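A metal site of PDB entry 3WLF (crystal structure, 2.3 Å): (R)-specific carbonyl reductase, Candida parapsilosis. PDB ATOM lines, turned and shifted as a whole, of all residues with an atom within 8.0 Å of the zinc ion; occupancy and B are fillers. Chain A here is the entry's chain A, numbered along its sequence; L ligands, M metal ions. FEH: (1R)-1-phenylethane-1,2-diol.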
ATOM      1  N   GLY A  47       1.224  20.336 -30.314  1.00  0.00           N
ATOM      2  CA  GLY A  47       1.801  19.191 -29.627  1.00  0.00           C
ATOM      3  C   GLY A  47       1.534  19.070 -28.136  1.00  0.00           C
ATOM      4  O   GLY A  47       1.042  19.998 -27.502  1.00  0.00           O
ATOM      5  N   LEU A  48       1.883  17.908 -27.596  1.00  0.00           N
ATOM      6  CA  LEU A  48       1.716  17.600 -26.172  1.00  0.00           C
ATOM      7  C   LEU A  48       2.977  16.954 -25.620  1.00  0.00           C
ATOM      8  O   LEU A  48       3.616  16.155 -26.307  1.00  0.00           O
ATOM      9  CB  LEU A  48       0.524  16.641 -25.989  1.00  0.00           C
ATOM     10  CG  LEU A  48       0.316  15.987 -24.616  1.00  0.00           C
ATOM     11  CD1 LEU A  48       0.015  17.033 -23.567  1.00  0.00           C
ATOM     12  CD2 LEU A  48      -0.819  14.984 -24.711  1.00  0.00           C
ATOM     13  N   CYS A  49       3.342  17.289 -24.386  1.00  0.00           N
ATOM     14  CA  CYS A  49       4.528  16.720 -23.750  1.00  0.00           C
ATOM     15  C   CYS A  49       4.425  16.834 -22.226  1.00  0.00           C
ATOM     16  O   CYS A  49       3.555  17.538 -21.713  1.00  0.00           O
ATOM     17  CB  CYS A  49       5.795  17.437 -24.232  1.00  0.00           C
ATOM     18  SG  CYS A  49       6.162  18.986 -23.366  1.00  0.00           S
ATOM     19  N   HIS A  50       5.321  16.147 -21.531  1.00  0.00           N
ATOM     20  CA  HIS A  50       5.341  16.140 -20.075  1.00  0.00           C
ATOM     21  C   HIS A  50       5.239  17.501 -19.403  1.00  0.00           C
ATOM     22  O   HIS A  50       4.677  17.625 -18.324  1.00  0.00           O
ATOM     23  CB  HIS A  50       6.599  15.427 -19.569  1.00  0.00           C
ATOM     24  CG  HIS A  50       6.570  13.947 -19.772  1.00  0.00           C
ATOM     25  ND1 HIS A  50       6.461  13.368 -21.013  1.00  0.00           N
ATOM     26  CD2 HIS A  50       6.634  12.927 -18.888  1.00  0.00           C
ATOM     27  CE1 HIS A  50       6.452  12.055 -20.890  1.00  0.00           C
ATOM     28  NE2 HIS A  50       6.567  11.761 -19.606  1.00  0.00           N
ATOM     29  N   SER A  51       5.775  18.531 -20.052  1.00  0.00           N
ATOM     30  CA  SER A  51       5.740  19.876 -19.487  1.00  0.00           C
ATOM     31  C   SER A  51       4.314  20.302 -19.121  1.00  0.00           C
ATOM     32  O   SER A  51       4.097  20.970 -18.115  1.00  0.00           O
ATOM     33  CB  SER A  51       6.340  20.882 -20.465  1.00  0.00           C
ATOM     34  OG  SER A  51       7.694  20.556 -20.740  1.00  0.00           O
ATOM     35  N   ASP A  52       3.348  19.905 -19.940  1.00  0.00           N
ATOM     36  CA  ASP A  52       1.953  20.240 -19.679  1.00  0.00           C
ATOM     37  C   ASP A  52       1.447  19.509 -18.442  1.00  0.00           C
ATOM     38  O   ASP A  52       0.620  20.026 -17.686  1.00  0.00           O
ATOM     39  CB  ASP A  52       1.070  19.882 -20.875  1.00  0.00           C
ATOM     40  CG  ASP A  52       1.401  20.710 -22.105  1.00  0.00           C
ATOM     41  OD1 ASP A  52       1.401  21.958 -22.004  1.00  0.00           O
ATOM     42  OD2 ASP A  52       1.657  20.112 -23.172  1.00  0.00           O
ATOM     43  N   GLY A  69      -1.106  24.352 -24.448  1.00  0.00           N
ATOM     44  CA  GLY A  69      -0.530  23.920 -25.702  1.00  0.00           C
ATOM     45  C   GLY A  69       0.572  24.890 -26.095  1.00  0.00           C
ATOM     46  O   GLY A  69       0.294  25.975 -26.607  1.00  0.00           O
ATOM     47  N   HIS A  70       1.822  24.517 -25.838  1.00  0.00           N
ATOM     48  CA  HIS A  70       2.964  25.378 -26.132  1.00  0.00           C
ATOM     49  C   HIS A  70       3.733  25.003 -27.395  1.00  0.00           C
ATOM     50  O   HIS A  70       4.775  25.589 -27.695  1.00  0.00           O
ATOM     51  CB  HIS A  70       3.928  25.392 -24.950  1.00  0.00           C
ATOM     52  CG  HIS A  70       4.349  24.029 -24.504  1.00  0.00           C
ATOM     53  ND1 HIS A  70       3.547  23.214 -23.738  1.00  0.00           N
ATOM     54  CD2 HIS A  70       5.496  23.330 -24.726  1.00  0.00           C
ATOM     55  CE1 HIS A  70       4.174  22.068 -23.509  1.00  0.00           C
ATOM     56  NE2 HIS A  70       5.362  22.115 -24.101  1.00  0.00           N
ATOM     57  N   GLU A  71       3.231  24.012 -28.131  1.00  0.00           N
ATOM     58  CA  GLU A  71       3.869  23.567 -29.364  1.00  0.00           C
ATOM     59  C   GLU A  71       2.935  23.884 -30.529  1.00  0.00           C
ATOM     60  O   GLU A  71       2.299  22.998 -31.088  1.00  0.00           O
ATOM     61  CB  GLU A  71       4.153  22.065 -29.281  1.00  0.00           C
ATOM     62  CG  GLU A  71       5.205  21.704 -28.236  1.00  0.00           C
ATOM     63  CD  GLU A  71       5.320  20.215 -27.988  1.00  0.00           C
ATOM     64  OE1 GLU A  71       5.356  19.438 -28.970  1.00  0.00           O
ATOM     65  OE2 GLU A  71       5.376  19.825 -26.804  1.00  0.00           O
ATOM     66  N   LEU A 124       1.443  28.409 -21.738  1.00  0.00           N
ATOM     67  CA  LEU A 124       1.974  28.297 -20.378  1.00  0.00           C
ATOM     68  C   LEU A 124       1.994  29.664 -19.723  1.00  0.00           C
ATOM     69  O   LEU A 124       3.056  30.201 -19.401  1.00  0.00           O
ATOM     70  CB  LEU A 124       3.391  27.708 -20.435  1.00  0.00           C
ATOM     71  CG  LEU A 124       3.458  26.271 -20.963  1.00  0.00           C
ATOM     72  CD1 LEU A 124       4.906  25.881 -21.230  1.00  0.00           C
ATOM     73  CD2 LEU A 124       2.832  25.336 -19.952  1.00  0.00           C
ATOM     74  N   TYR A 130      -4.191  24.778 -28.003  1.00  0.00           N
ATOM     75  CA  TYR A 130      -5.304  23.857 -27.802  1.00  0.00           C
ATOM     76  C   TYR A 130      -6.628  24.568 -28.074  1.00  0.00           C
ATOM     77  O   TYR A 130      -7.550  24.519 -27.260  1.00  0.00           O
ATOM     78  CB  TYR A 130      -5.309  23.277 -26.388  1.00  0.00           C
ATOM     79  CG  TYR A 130      -4.176  22.319 -26.088  1.00  0.00           C
ATOM     80  CD1 TYR A 130      -3.654  21.502 -27.079  1.00  0.00           C
ATOM     81  CD2 TYR A 130      -3.658  22.213 -24.800  1.00  0.00           C
ATOM     82  CE1 TYR A 130      -2.616  20.605 -26.804  1.00  0.00           C
ATOM     83  CE2 TYR A 130      -2.628  21.318 -24.514  1.00  0.00           C
ATOM     84  CZ  TYR A 130      -2.112  20.519 -25.521  1.00  0.00           C
ATOM     85  OH  TYR A 130      -1.099  19.634 -25.249  1.00  0.00           O
ATOM     86  N   ALA A 155       5.161  21.703 -35.669  1.00  0.00           N
ATOM     87  CA  ALA A 155       4.731  21.745 -34.277  1.00  0.00           C
ATOM     88  C   ALA A 155       5.587  20.827 -33.419  1.00  0.00           C
ATOM     89  O   ALA A 155       5.977  21.189 -32.319  1.00  0.00           O
ATOM     90  CB  ALA A 155       3.270  21.343 -34.178  1.00  0.00           C
ATOM     91  N   THR A 158       8.840  22.599 -32.437  1.00  0.00           N
ATOM     92  CA  THR A 158       8.808  23.784 -31.582  1.00  0.00           C
ATOM     93  C   THR A 158       9.372  23.553 -30.180  1.00  0.00           C
ATOM     94  O   THR A 158       9.655  24.511 -29.459  1.00  0.00           O
ATOM     95  CB  THR A 158       7.365  24.324 -31.439  1.00  0.00           C
ATOM     96  OG1 THR A 158       6.537  23.310 -30.857  1.00  0.00           O
ATOM     97  CG2 THR A 158       6.814  24.709 -32.800  1.00  0.00           C
ATOM     98  N   ASP A 159       9.535  22.298 -29.790  1.00  0.00           N
ATOM     99  CA  ASP A 159      10.059  21.997 -28.469  1.00  0.00           C
ATOM    100  C   ASP A 159      10.954  20.757 -28.453  1.00  0.00           C
ATOM    101  O   ASP A 159      12.079  20.820 -27.954  1.00  0.00           O
ATOM    102  CB  ASP A 159       8.892  21.821 -27.480  1.00  0.00           C
ATOM    103  CG  ASP A 159       9.354  21.645 -26.056  1.00  0.00           C
ATOM    104  OD1 ASP A 159      10.407  22.204 -25.692  1.00  0.00           O
ATOM    105  OD2 ASP A 159       8.654  20.961 -25.278  1.00  0.00           O
ATOM    106  N   ALA A 160      10.460  19.658 -29.008  1.00  0.00           N
ATOM    107  CA  ALA A 160      11.228  18.420 -29.042  1.00  0.00           C
ATOM    108  C   ALA A 160      12.541  18.558 -29.803  1.00  0.00           C
ATOM    109  O   ALA A 160      13.476  17.794 -29.580  1.00  0.00           O
ATOM    110  CB  ALA A 160      10.380  17.302 -29.670  1.00  0.00           C
ATOM    111  N   THR A 163      14.545  22.738 -28.208  1.00  0.00           N
ATOM    112  CA  THR A 163      15.261  22.677 -26.949  1.00  0.00           C
ATOM    113  C   THR A 163      16.638  22.022 -27.070  1.00  0.00           C
ATOM    114  O   THR A 163      17.650  22.638 -26.735  1.00  0.00           O
ATOM    115  CB  THR A 163      14.429  21.934 -25.879  1.00  0.00           C
ATOM    116  OG1 THR A 163      13.222  22.666 -25.617  1.00  0.00           O
ATOM    117  CG2 THR A 163      15.220  21.793 -24.580  1.00  0.00           C
ATOM    118  N   LEU A 187      13.663  13.948 -26.047  1.00  0.00           N
ATOM    119  CA  LEU A 187      14.573  14.964 -26.570  1.00  0.00           C
ATOM    120  C   LEU A 187      15.968  14.401 -26.815  1.00  0.00           C
ATOM    121  O   LEU A 187      16.762  14.977 -27.552  1.00  0.00           O
ATOM    122  CB  LEU A 187      14.650  16.168 -25.629  1.00  0.00           C
ATOM    123  CG  LEU A 187      13.466  17.152 -25.634  1.00  0.00           C
ATOM    124  CD1 LEU A 187      12.179  16.432 -25.264  1.00  0.00           C
ATOM    125  CD2 LEU A 187      13.753  18.277 -24.651  1.00  0.00           C
ATOM    126  N   TRP A 291      14.649  25.878 -23.228  1.00  0.00           N
ATOM    127  CA  TRP A 291      13.912  25.944 -24.493  1.00  0.00           C
ATOM    128  C   TRP A 291      14.822  26.389 -25.639  1.00  0.00           C
ATOM    129  O   TRP A 291      15.887  25.812 -25.868  1.00  0.00           O
ATOM    130  CB  TRP A 291      12.741  26.917 -24.373  1.00  0.00           C
ATOM    131  CG  TRP A 291      11.485  26.456 -25.042  1.00  0.00           C
ATOM    132  CD1 TRP A 291      11.384  25.773 -26.227  1.00  0.00           C
ATOM    133  CD2 TRP A 291      10.144  26.666 -24.591  1.00  0.00           C
ATOM    134  NE1 TRP A 291      10.069  25.554 -26.533  1.00  0.00           N
ATOM    135  CE2 TRP A 291       9.278  26.083 -25.548  1.00  0.00           C
ATOM    136  CE3 TRP A 291       9.582  27.296 -23.470  1.00  0.00           C
ATOM    137  CZ2 TRP A 291       7.888  26.118 -25.417  1.00  0.00           C
ATOM    138  CZ3 TRP A 291       8.193  27.318 -23.336  1.00  0.00           C
ATOM    139  CH2 TRP A 291       7.365  26.726 -24.309  1.00  0.00           C
ATOM    140  N   ARG A 336       6.105  12.006 -29.802  1.00  0.00           N
ATOM    141  CA  ARG A 336       5.073  12.991 -29.528  1.00  0.00           C
ATOM    142  C   ARG A 336       3.848  12.781 -30.405  1.00  0.00           C
ATOM    143  O   ARG A 336       3.884  12.065 -31.405  1.00  0.00           O
ATOM    144  CB  ARG A 336       5.606  14.411 -29.741  1.00  0.00           C
ATOM    145  CG  ARG A 336       6.252  15.038 -28.519  1.00  0.00           C
ATOM    146  CD  ARG A 336       6.660  16.477 -28.809  1.00  0.00           C
ATOM    147  NE  ARG A 336       7.112  17.186 -27.618  1.00  0.00           N
ATOM    148  CZ  ARG A 336       8.153  16.816 -26.870  1.00  0.00           C
ATOM    149  NH1 ARG A 336       8.857  15.740 -27.195  1.00  0.00           N
ATOM    150  NH2 ARG A 336       8.487  17.527 -25.811  1.00  0.00           N
HETATM  151  C4  FEH L   1       8.518  24.529 -20.422  1.00  0.00           C
HETATM  152  C5  FEH L   1       7.814  24.923 -19.239  1.00  0.00           C
HETATM  153  C6  FEH L   1       8.020  24.198 -18.010  1.00  0.00           C
HETATM  154  C7  FEH L   1       8.923  23.078 -17.970  1.00  0.00           C
HETATM  155  C8  FEH L   1       9.627  22.684 -19.153  1.00  0.00           C
HETATM  156  C2  FEH L   1       9.429  23.407 -20.393  1.00  0.00           C
HETATM  157  C1  FEH L   1      10.154  22.955 -21.518  1.00  0.00           C
HETATM  158  O1  FEH L   1       9.040  22.516 -22.307  1.00  0.00           O
HETATM  159  C3  FEH L   1      11.077  23.967 -22.251  1.00  0.00           C
HETATM  160  O2  FEH L   1      12.193  23.642 -23.088  1.00  0.00           O
HETATM  161 ZN    ZN M   1       6.521  20.679 -25.054  1.00  0.00          ZN
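A ring nitrogen (ND1) of His 70 sits at hydrogen-bond distance from the side-chain carboxylate (OD1) of Asp 52, 3.0 Å away. OD2 of Asp 159 lies close to NH2 of Arg 336, at 3.5 Å. The indole nitrogen (NE1) of Trp 291 sits at hydrogen-bond distance from the side-chain carboxylate (OD1) of Asp 159 (3.5 Å). OD1 of Asp 159 sits at hydrogen-bond distance from OG1 of Thr 163 (2.9 Å). The side-chain carboxylate (OE1) of Glu 71 is in salt-bridge range of the guanidinium group (NE) of Arg 336 (3.2 Å). The backbone NH (N) of Gly 47 is in hydrogen-bond range of the backbone carbonyl oxygen (O) of Glu 71 (3.0 Å). The side-chain sulfur of Cys 49 lies close to the guanidinium group of Arg 336. SG of Cys 49 lies close to N of Ser 51 (3.4 Å).
Residues that only touch the zinc ion: Arg 336. Of the 19 residues printed, 5 come within 4 Å of the zinc ion.
OD1 of Asp 159 lies within hydrogen-bond range of O2 of the ligand. OG of Ser 51 sits at hydrogen-bond distance from O1 of the ligand, 2.8 Å away. N of Trp 291 sits close to O2 of the ligand, 3.3 Å away. OG1 of Thr 163 sits at hydrogen-bond distance from O2 of the ligand (2.9 Å).
The zinc ion is bound by NE2 of His 70 (2.1 Å), OD2 of Asp 159 (2.2 Å), OE2 of Glu 71 (2.3 Å) and SG of Cys 49 (2.4 Å).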
